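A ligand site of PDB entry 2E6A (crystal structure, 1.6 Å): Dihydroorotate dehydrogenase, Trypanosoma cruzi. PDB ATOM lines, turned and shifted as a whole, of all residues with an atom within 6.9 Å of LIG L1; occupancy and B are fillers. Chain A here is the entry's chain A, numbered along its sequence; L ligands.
O of Ala 21 lies close to O3 of LG2 L2 (2.8 Å).
An oxygen (O3) of LIG L1 sits at hydrogen-bond distance from the backbone NH (N) of Leu 73 (2.8 Å).
The side-chain amide nitrogen (ND2) of Asn 196 lies within hydrogen-bond range of an oxygen (O1) of LG2 L2 (3.5 Å).
The side-chain amide oxygen (OD1) of Asn 196 sits at hydrogen-bond distance from a nitrogen (N2) of LIG L1 (2.7 Å).
N1 of LIG L1 sits at hydrogen-bond distance from OD1 of Asn 69, 2.9 Å away.
An oxygen (O3) of LIG L1 is in salt-bridge range of the side-chain amino group (NZ) of Lys 45, 2.9 Å away.
An oxygen (O2) of LG2 L2 is in hydrogen-bond range of the side-chain amino group (NZ) of Lys 45 (2.8 Å).
O1 of LIG L1 lies within hydrogen-bond range of OG of Ser 197 (2.8 Å).
N of Met 71 lies within hydrogen-bond range of O4 of LIG L1 (3.0 Å).
The side-chain amide nitrogen (ND2) of Asn 134 lies within hydrogen-bond range of an oxygen (O4) of LIG L1.
O2 of LIG L1 lies within hydrogen-bond range of ND2 of Asn 129 (2.9 Å).
A nitrogen (N2) of LG2 L2 is in hydrogen-bond range of the side-chain hydroxyl (OG) of Ser 46, at 2.8 Å.
The backbone NH (N) of Ser 46 is in hydrogen-bond range of an oxygen (O2) of LG2 L2, 3.3 Å away.
O4 of LIG L1 is in hydrogen-bond range of N of Gly 72 (2.8 Å).
An oxygen (O1) of LG2 L2 sits at hydrogen-bond distance from the side-chain amide nitrogen of Asn 129, 3.2 Å away.
NZ of Lys 166 sits at hydrogen-bond distance from O3 of LG2 L2 (2.9 Å).
O2 of LIG L1 lies close to N2 of LG2 L2.
OG of Ser 197 lies within hydrogen-bond range of OD1 of Asn 196, 3.5 Å away.
The backbone carbonyl oxygen of Met 71 lies within hydrogen-bond range of the backbone NH of Asn 55.
OD1 of Asn 129 is in hydrogen-bond range of ND2 of Asn 196 (3.4 Å).
The backbone NH (N) of Ser 70 sits at hydrogen-bond distance from the backbone carbonyl oxygen (O) of Arg 59 (2.8 Å).
The side-chain amide nitrogen (ND2) of Asn 129 is in hydrogen-bond range of the side-chain hydroxyl (OG) of Ser 46, 3.1 Å away.
The side-chain amide nitrogen (ND2) of Asn 196 sits at hydrogen-bond distance from the side-chain hydroxyl (OG) of Ser 131 (2.9 Å).
The backbone NH of Cys 132 is in hydrogen-bond range of the side-chain amide oxygen of Asn 129.
The backbone carbonyl oxygen (O) of Asn 134 lies within hydrogen-bond range of the side-chain amide nitrogen (ND2) of Asn 55, 3.0 Å away.
Merely in contact with LIG L1: Cys 132, Pro 133, Pro 74 and Ser 70.
Hydrophobic or aromatic side chains that line LIG L1: Met 71, Leu 73, Pro 74 and Pro 133.
Within 4 Å of LIG L1: Lys 45, Asn 69, Ser 70, Met 71, Gly 72, Leu 73, Pro 74, Asn 129, Cys 132, Pro 133, Asn 134, Asn 196 and Ser 197.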
ATOM      1  N   ALA A  21     -12.577 -20.505   1.905  1.00  0.00           N
ATOM      2  CA  ALA A  21     -11.807 -21.682   2.306  1.00  0.00           C
ATOM      3  C   ALA A  21     -12.325 -22.939   1.628  1.00  0.00           C
ATOM      4  O   ALA A  21     -13.529 -23.114   1.474  1.00  0.00           O
ATOM      5  CB  ALA A  21     -11.795 -21.850   3.816  1.00  0.00           C
ATOM      6  N   GLY A  22     -11.407 -23.792   1.197  1.00  0.00           N
ATOM      7  CA  GLY A  22     -11.791 -25.069   0.585  1.00  0.00           C
ATOM      8  C   GLY A  22     -11.829 -25.022  -0.925  1.00  0.00           C
ATOM      9  O   GLY A  22     -11.724 -26.076  -1.573  1.00  0.00           O
ATOM     10  N   LYS A  45      -7.047 -24.468   2.436  1.00  0.00           N
ATOM     11  CA  LYS A  45      -8.056 -25.485   2.770  1.00  0.00           C
ATOM     12  C   LYS A  45      -8.083 -25.743   4.277  1.00  0.00           C
ATOM     13  O   LYS A  45      -7.024 -25.896   4.894  1.00  0.00           O
ATOM     14  CB  LYS A  45      -7.678 -26.792   2.038  1.00  0.00           C
ATOM     15  CG  LYS A  45      -8.479 -28.035   2.483  1.00  0.00           C
ATOM     16  CD  LYS A  45      -9.947 -27.939   2.068  1.00  0.00           C
ATOM     17  CE  LYS A  45     -10.802 -29.008   2.756  1.00  0.00           C
ATOM     18  NZ  LYS A  45     -12.259 -28.777   2.395  1.00  0.00           N
ATOM     19  N   SER A  46      -9.272 -25.847   4.870  1.00  0.00           N
ATOM     20  CA  SER A  46      -9.338 -26.191   6.304  1.00  0.00           C
ATOM     21  C   SER A  46      -8.628 -27.512   6.530  1.00  0.00           C
ATOM     22  O   SER A  46      -8.935 -28.525   5.868  1.00  0.00           O
ATOM     23  CB  SER A  46     -10.780 -26.318   6.795  1.00  0.00           C
ATOM     24  OG  SER A  46     -11.365 -25.054   6.842  1.00  0.00           O
ATOM     25  N   ASN A  55     -14.370 -37.660   2.193  1.00  0.00           N
ATOM     26  CA  ASN A  55     -15.511 -38.527   1.944  1.00  0.00           C
ATOM     27  C   ASN A  55     -15.461 -39.156   0.523  1.00  0.00           C
ATOM     28  O   ASN A  55     -14.741 -38.687  -0.346  1.00  0.00           O
ATOM     29  CB  ASN A  55     -16.821 -37.724   2.106  1.00  0.00           C
ATOM     30  CG  ASN A  55     -17.113 -37.337   3.555  1.00  0.00           C
ATOM     31  OD1 ASN A  55     -16.554 -37.906   4.520  1.00  0.00           O
ATOM     32  ND2 ASN A  55     -18.011 -36.378   3.718  1.00  0.00           N
ATOM     33  N   ARG A  59     -18.570 -36.091  -4.585  1.00  0.00           N
ATOM     34  CA  ARG A  59     -18.791 -35.346  -3.351  1.00  0.00           C
ATOM     35  C   ARG A  59     -18.952 -33.845  -3.555  1.00  0.00           C
ATOM     36  O   ARG A  59     -19.122 -33.090  -2.589  1.00  0.00           O
ATOM     37  CB  ARG A  59     -17.677 -35.667  -2.342  1.00  0.00           C
ATOM     38  CG  ARG A  59     -16.300 -35.203  -2.763  1.00  0.00           C
ATOM     39  CD  ARG A  59     -15.204 -35.959  -2.048  1.00  0.00           C
ATOM     40  NE  ARG A  59     -13.875 -35.488  -2.453  1.00  0.00           N
ATOM     41  CZ  ARG A  59     -12.737 -35.889  -1.880  1.00  0.00           C
ATOM     42  NH1 ARG A  59     -12.763 -36.769  -0.878  1.00  0.00           N
ATOM     43  NH2 ARG A  59     -11.587 -35.397  -2.305  1.00  0.00           N
ATOM     44  N   ASN A  69     -21.959 -29.890  -1.536  1.00  0.00           N
ATOM     45  CA  ASN A  69     -20.692 -30.588  -1.317  1.00  0.00           C
ATOM     46  C   ASN A  69     -20.681 -31.336  -0.018  1.00  0.00           C
ATOM     47  O   ASN A  69     -21.245 -30.879   0.970  1.00  0.00           O
ATOM     48  CB  ASN A  69     -19.479 -29.624  -1.383  1.00  0.00           C
ATOM     49  CG  ASN A  69     -19.124 -28.992  -0.031  1.00  0.00           C
ATOM     50  OD1 ASN A  69     -18.429 -29.580   0.804  1.00  0.00           O
ATOM     51  ND2 ASN A  69     -19.601 -27.771   0.182  1.00  0.00           N
ATOM     52  N   SER A  70     -20.053 -32.501  -0.030  1.00  0.00           N
ATOM     53  CA  SER A  70     -19.705 -33.186   1.208  1.00  0.00           C
ATOM     54  C   SER A  70     -18.272 -33.665   1.085  1.00  0.00           C
ATOM     55  O   SER A  70     -17.988 -34.865   1.057  1.00  0.00           O
ATOM     56  CB  SER A  70     -20.663 -34.346   1.479  1.00  0.00           C
ATOM     57  OG  SER A  70     -20.364 -34.934   2.751  1.00  0.00           O
ATOM     58  N   MET A  71     -17.340 -32.716   0.991  1.00  0.00           N
ATOM     59  CA  MET A  71     -15.944 -33.097   0.736  1.00  0.00           C
ATOM     60  C   MET A  71     -15.372 -33.964   1.868  1.00  0.00           C
ATOM     61  O   MET A  71     -14.693 -34.955   1.597  1.00  0.00           O
ATOM     62  CB  MET A  71     -15.065 -31.868   0.506  1.00  0.00           C
ATOM     63  CG  MET A  71     -15.617 -30.856  -0.488  1.00  0.00           C
ATOM     64  SD  MET A  71     -15.813 -31.536  -2.141  1.00  0.00           S
ATOM     65  CE  MET A  71     -14.106 -31.843  -2.584  1.00  0.00           C
ATOM     66  N   GLY A  72     -15.649 -33.578   3.122  1.00  0.00           N
ATOM     67  CA  GLY A  72     -15.209 -34.332   4.308  1.00  0.00           C
ATOM     68  C   GLY A  72     -13.800 -33.973   4.732  1.00  0.00           C
ATOM     69  O   GLY A  72     -13.045 -34.825   5.216  1.00  0.00           O
ATOM     70  N   LEU A  73     -13.437 -32.709   4.517  1.00  0.00           N
ATOM     71  CA  LEU A  73     -12.105 -32.170   4.880  1.00  0.00           C
ATOM     72  C   LEU A  73     -10.939 -32.956   4.275  1.00  0.00           C
ATOM     73  O   LEU A  73      -9.977 -33.291   4.979  1.00  0.00           O
ATOM     74  CB  LEU A  73     -11.959 -32.038   6.403  1.00  0.00           C
ATOM     75  CG  LEU A  73     -12.873 -31.030   7.088  1.00  0.00           C
ATOM     76  CD1 LEU A  73     -12.766 -31.169   8.605  1.00  0.00           C
ATOM     77  CD2 LEU A  73     -12.526 -29.611   6.658  1.00  0.00           C
ATOM     78  N   PRO A  74     -10.993 -33.207   2.945  1.00  0.00           N
ATOM     79  CA  PRO A  74      -9.806 -33.805   2.332  1.00  0.00           C
ATOM     80  C   PRO A  74      -8.731 -32.739   2.339  1.00  0.00           C
ATOM     81  O   PRO A  74      -8.988 -31.595   1.955  1.00  0.00           O
ATOM     82  CB  PRO A  74     -10.256 -34.114   0.896  1.00  0.00           C
ATOM     83  CG  PRO A  74     -11.392 -33.185   0.626  1.00  0.00           C
ATOM     84  CD  PRO A  74     -12.041 -32.886   1.960  1.00  0.00           C
ATOM     85  N   SER A 101      -9.485 -26.873  10.921  1.00  0.00           N
ATOM     86  CA  SER A 101     -10.758 -27.479  11.295  1.00  0.00           C
ATOM     87  C   SER A 101     -10.529 -28.811  11.974  1.00  0.00           C
ATOM     88  O   SER A 101     -10.935 -29.847  11.470  1.00  0.00           O
ATOM     89  CB  SER A 101     -11.686 -27.632  10.067  1.00  0.00           C
ATOM     90  OG  SER A 101     -13.009 -27.961  10.478  1.00  0.00           O
ATOM     91  N   ASN A 129     -12.183 -22.787  11.883  1.00  0.00           N
ATOM     92  CA  ASN A 129     -13.437 -23.258  11.279  1.00  0.00           C
ATOM     93  C   ASN A 129     -14.321 -23.978  12.311  1.00  0.00           C
ATOM     94  O   ASN A 129     -14.025 -25.092  12.717  1.00  0.00           O
ATOM     95  CB  ASN A 129     -13.104 -24.178  10.094  1.00  0.00           C
ATOM     96  CG  ASN A 129     -14.316 -24.638   9.335  1.00  0.00           C
ATOM     97  OD1 ASN A 129     -15.447 -24.338   9.713  1.00  0.00           O
ATOM     98  ND2 ASN A 129     -14.095 -25.365   8.237  1.00  0.00           N
ATOM     99  N   SER A 131     -17.616 -24.586  11.691  1.00  0.00           N
ATOM    100  CA  SER A 131     -18.865 -24.768  10.957  1.00  0.00           C
ATOM    101  C   SER A 131     -18.837 -25.832   9.835  1.00  0.00           C
ATOM    102  O   SER A 131     -19.722 -25.856   8.984  1.00  0.00           O
ATOM    103  CB  SER A 131     -19.334 -23.406  10.429  1.00  0.00           C
ATOM    104  OG  SER A 131     -18.257 -22.697   9.827  1.00  0.00           O
ATOM    105  N   CYS A 132     -17.860 -26.729   9.860  1.00  0.00           N
ATOM    106  CA  CYS A 132     -17.891 -27.815   8.872  1.00  0.00           C
ATOM    107  C   CYS A 132     -19.143 -28.685   9.072  1.00  0.00           C
ATOM    108  O   CYS A 132     -19.344 -29.225  10.165  1.00  0.00           O
ATOM    109  CB  CYS A 132     -16.626 -28.664   8.981  1.00  0.00           C
ATOM    110  SG  CYS A 132     -16.689 -30.124   7.885  1.00  0.00           S
ATOM    111  N   PRO A 133     -20.007 -28.790   8.030  1.00  0.00           N
ATOM    112  CA  PRO A 133     -21.221 -29.592   8.158  1.00  0.00           C
ATOM    113  C   PRO A 133     -21.147 -31.006   7.558  1.00  0.00           C
ATOM    114  O   PRO A 133     -22.199 -31.649   7.394  1.00  0.00           O
ATOM    115  CB  PRO A 133     -22.231 -28.774   7.355  1.00  0.00           C
ATOM    116  CG  PRO A 133     -21.371 -28.225   6.160  1.00  0.00           C
ATOM    117  CD  PRO A 133     -19.937 -28.114   6.710  1.00  0.00           C
ATOM    118  N   ASN A 134     -19.950 -31.456   7.197  1.00  0.00           N
ATOM    119  CA  ASN A 134     -19.807 -32.640   6.338  1.00  0.00           C
ATOM    120  C   ASN A 134     -19.055 -33.869   6.874  1.00  0.00           C
ATOM    121  O   ASN A 134     -18.933 -34.861   6.155  1.00  0.00           O
ATOM    122  CB  ASN A 134     -19.167 -32.254   5.001  1.00  0.00           C
ATOM    123  CG  ASN A 134     -20.029 -31.317   4.206  1.00  0.00           C
ATOM    124  OD1 ASN A 134     -21.271 -31.416   4.203  1.00  0.00           O
ATOM    125  ND2 ASN A 134     -19.377 -30.408   3.477  1.00  0.00           N
ATOM    126  N   VAL A 135     -18.536 -33.798   8.095  1.00  0.00           N
ATOM    127  CA  VAL A 135     -17.831 -34.973   8.625  1.00  0.00           C
ATOM    128  C   VAL A 135     -18.842 -35.828   9.377  1.00  0.00           C
ATOM    129  O   VAL A 135     -19.511 -35.320  10.282  1.00  0.00           O
ATOM    130  CB  VAL A 135     -16.618 -34.598   9.500  1.00  0.00           C
ATOM    131  CG1 VAL A 135     -16.005 -35.845  10.138  1.00  0.00           C
ATOM    132  CG2 VAL A 135     -15.551 -33.889   8.664  1.00  0.00           C
ATOM    133  N   LYS A 166     -14.742 -18.937  11.295  1.00  0.00           N
ATOM    134  CA  LYS A 166     -15.689 -19.202  10.210  1.00  0.00           C
ATOM    135  C   LYS A 166     -16.978 -19.750  10.822  1.00  0.00           C
ATOM    136  O   LYS A 166     -16.957 -20.815  11.448  1.00  0.00           O
ATOM    137  CB  LYS A 166     -15.070 -20.216   9.215  1.00  0.00           C
ATOM    138  CG  LYS A 166     -15.980 -20.573   8.029  1.00  0.00           C
ATOM    139  CD  LYS A 166     -16.071 -19.415   7.039  1.00  0.00           C
ATOM    140  CE  LYS A 166     -16.659 -19.848   5.695  1.00  0.00           C
ATOM    141  NZ  LYS A 166     -15.766 -20.720   4.895  1.00  0.00           N
ATOM    142  N   ASN A 196     -20.264 -20.154   6.315  1.00  0.00           N
ATOM    143  CA  ASN A 196     -20.013 -21.467   5.738  1.00  0.00           C
ATOM    144  C   ASN A 196     -21.257 -21.935   4.951  1.00  0.00           C
ATOM    145  O   ASN A 196     -22.286 -21.250   4.921  1.00  0.00           O
ATOM    146  CB  ASN A 196     -19.675 -22.462   6.858  1.00  0.00           C
ATOM    147  CG  ASN A 196     -18.704 -23.538   6.411  1.00  0.00           C
ATOM    148  OD1 ASN A 196     -18.872 -24.165   5.359  1.00  0.00           O
ATOM    149  ND2 ASN A 196     -17.677 -23.761   7.222  1.00  0.00           N
ATOM    150  N   SER A 197     -21.148 -23.099   4.313  1.00  0.00           N
ATOM    151  CA  SER A 197     -22.254 -23.616   3.513  1.00  0.00           C
ATOM    152  C   SER A 197     -23.477 -23.868   4.378  1.00  0.00           C
ATOM    153  O   SER A 197     -23.375 -24.113   5.610  1.00  0.00           O
ATOM    154  CB  SER A 197     -21.824 -24.890   2.783  1.00  0.00           C
ATOM    155  OG  SER A 197     -21.441 -25.875   3.717  1.00  0.00           O
ATOM    156  N   VAL A 198     -24.641 -23.792   3.747  1.00  0.00           N
ATOM    157  CA  VAL A 198     -25.903 -24.033   4.444  1.00  0.00           C
ATOM    158  C   VAL A 198     -26.033 -25.549   4.590  1.00  0.00           C
ATOM    159  O   VAL A 198     -26.199 -26.274   3.601  1.00  0.00           O
ATOM    160  CB  VAL A 198     -27.070 -23.373   3.687  1.00  0.00           C
ATOM    161  CG1 VAL A 198     -28.402 -23.866   4.211  1.00  0.00           C
ATOM    162  CG2 VAL A 198     -26.989 -21.839   3.815  1.00  0.00           C
ATOM    163  N   GLY A 220     -25.555 -32.663   1.952  1.00  0.00           N
ATOM    164  CA  GLY A 220     -24.320 -31.876   1.901  1.00  0.00           C
ATOM    165  C   GLY A 220     -24.579 -30.394   1.989  1.00  0.00           C
ATOM    166  O   GLY A 220     -25.728 -29.962   1.924  1.00  0.00           O
ATOM    167  N   GLY A 221     -23.505 -29.627   2.175  1.00  0.00           N
ATOM    168  CA  GLY A 221     -23.625 -28.174   2.378  1.00  0.00           C
ATOM    169  C   GLY A 221     -23.922 -27.466   1.077  1.00  0.00           C
ATOM    170  O   GLY A 221     -23.321 -27.782   0.052  1.00  0.00           O
ATOM    171  N   LEU A 222     -24.823 -26.480   1.133  1.00  0.00           N
ATOM    172  CA  LEU A 222     -25.210 -25.696  -0.042  1.00  0.00           C
ATOM    173  C   LEU A 222     -24.443 -24.383  -0.144  1.00  0.00           C
ATOM    174  O   LEU A 222     -24.249 -23.676   0.850  1.00  0.00           O
ATOM    175  CB  LEU A 222     -26.716 -25.384  -0.004  1.00  0.00           C
ATOM    176  CG  LEU A 222     -27.666 -26.573   0.148  1.00  0.00           C
ATOM    177  CD1 LEU A 222     -29.104 -26.067   0.359  1.00  0.00           C
ATOM    178  CD2 LEU A 222     -27.591 -27.503  -1.056  1.00  0.00           C
HETATM  179  N1  LIG L   1     -17.312 -28.258   3.144  1.00  0.00           N
HETATM  180  C1  LIG L   1     -17.947 -27.130   3.518  1.00  0.00           C
HETATM  181  O1  LIG L   1     -18.930 -26.700   2.854  1.00  0.00           O
HETATM  182  N2  LIG L   1     -17.537 -26.448   4.620  1.00  0.00           N
HETATM  183  C2  LIG L   1     -16.511 -26.889   5.369  1.00  0.00           C
HETATM  184  O2  LIG L   1     -16.176 -26.250   6.377  1.00  0.00           O
HETATM  185  C3  LIG L   1     -15.839 -28.077   5.032  1.00  0.00           C
HETATM  186  C4  LIG L   1     -16.254 -28.718   3.867  1.00  0.00           C
HETATM  187  C5  LIG L   1     -15.660 -30.026   3.504  1.00  0.00           C
HETATM  188  O3  LIG L   1     -14.424 -30.266   3.516  1.00  0.00           O
HETATM  189  O4  LIG L   1     -16.534 -30.894   3.291  1.00  0.00           O
HETATM  190  N1  LG2 L   2     -15.358 -23.754   4.153  1.00  0.00           N
HETATM  191  C1  LG2 L   2     -14.415 -23.851   5.129  1.00  0.00           C
HETATM  192  O1  LG2 L   2     -14.456 -23.061   6.099  1.00  0.00           O
HETATM  193  N2  LG2 L   2     -13.426 -24.796   5.021  1.00  0.00           N
HETATM  194  C2  LG2 L   2     -13.341 -25.673   3.959  1.00  0.00           C
HETATM  195  O2  LG2 L   2     -12.322 -26.395   3.840  1.00  0.00           O
HETATM  196  C3  LG2 L   2     -14.307 -25.563   2.958  1.00  0.00           C
HETATM  197  N3  LG2 L   2     -14.283 -26.399   1.848  1.00  0.00           N
HETATM  198  C4  LG2 L   2     -15.226 -26.240   0.843  1.00  0.00           C
HETATM  199  C5  LG2 L   2     -15.166 -27.086  -0.262  1.00  0.00           C
HETATM  200  C6  LG2 L   2     -16.104 -26.946  -1.281  1.00  0.00           C
HETATM  201  C7  LG2 L   2     -15.795 -27.618  -2.591  1.00  0.00           C
HETATM  202  C8  LG2 L   2     -17.115 -25.975  -1.187  1.00  0.00           C
HETATM  203  C9  LG2 L   2     -17.849 -25.520  -2.422  1.00  0.00           C
HETATM  204  C10 LG2 L   2     -17.182 -25.153  -0.066  1.00  0.00           C
HETATM  205  C11 LG2 L   2     -16.222 -25.272   0.945  1.00  0.00           C
HETATM  206  N4  LG2 L   2     -16.283 -24.487   2.069  1.00  0.00           N
HETATM  207  C12 LG2 L   2     -15.318 -24.594   3.061  1.00  0.00           C
HETATM  208  C13 LG2 L   2     -17.423 -23.534   2.305  1.00  0.00           C
HETATM  209  C14 LG2 L   2     -17.048 -22.242   1.572  1.00  0.00           C
HETATM  210  O3  LG2 L   2     -15.884 -21.683   2.160  1.00  0.00           O
HETATM  211  C15 LG2 L   2     -18.164 -21.199   1.659  1.00  0.00           C
HETATM  212  O4  LG2 L   2     -18.345 -20.839   3.021  1.00  0.00           O
HETATM  213  C16 LG2 L   2     -19.489 -21.713   1.075  1.00  0.00           C
HETATM  214  O5  LG2 L   2     -19.270 -22.506  -0.096  1.00  0.00           O
HETATM  215  C17 LG2 L   2     -20.462 -20.583   0.715  1.00  0.00           C
HETATM  216  O6  LG2 L   2     -19.908 -19.669  -0.208  1.00  0.00           O
HETATM  217  P1  LG2 L   2     -20.367 -19.704  -1.765  1.00  0.00           P
HETATM  218  O7  LG2 L   2     -21.840 -19.423  -1.808  1.00  0.00           O
HETATM  219  O8  LG2 L   2     -19.511 -18.678  -2.492  1.00  0.00           O
HETATM  220  O9  LG2 L   2     -20.061 -21.084  -2.268  1.00  0.00           O
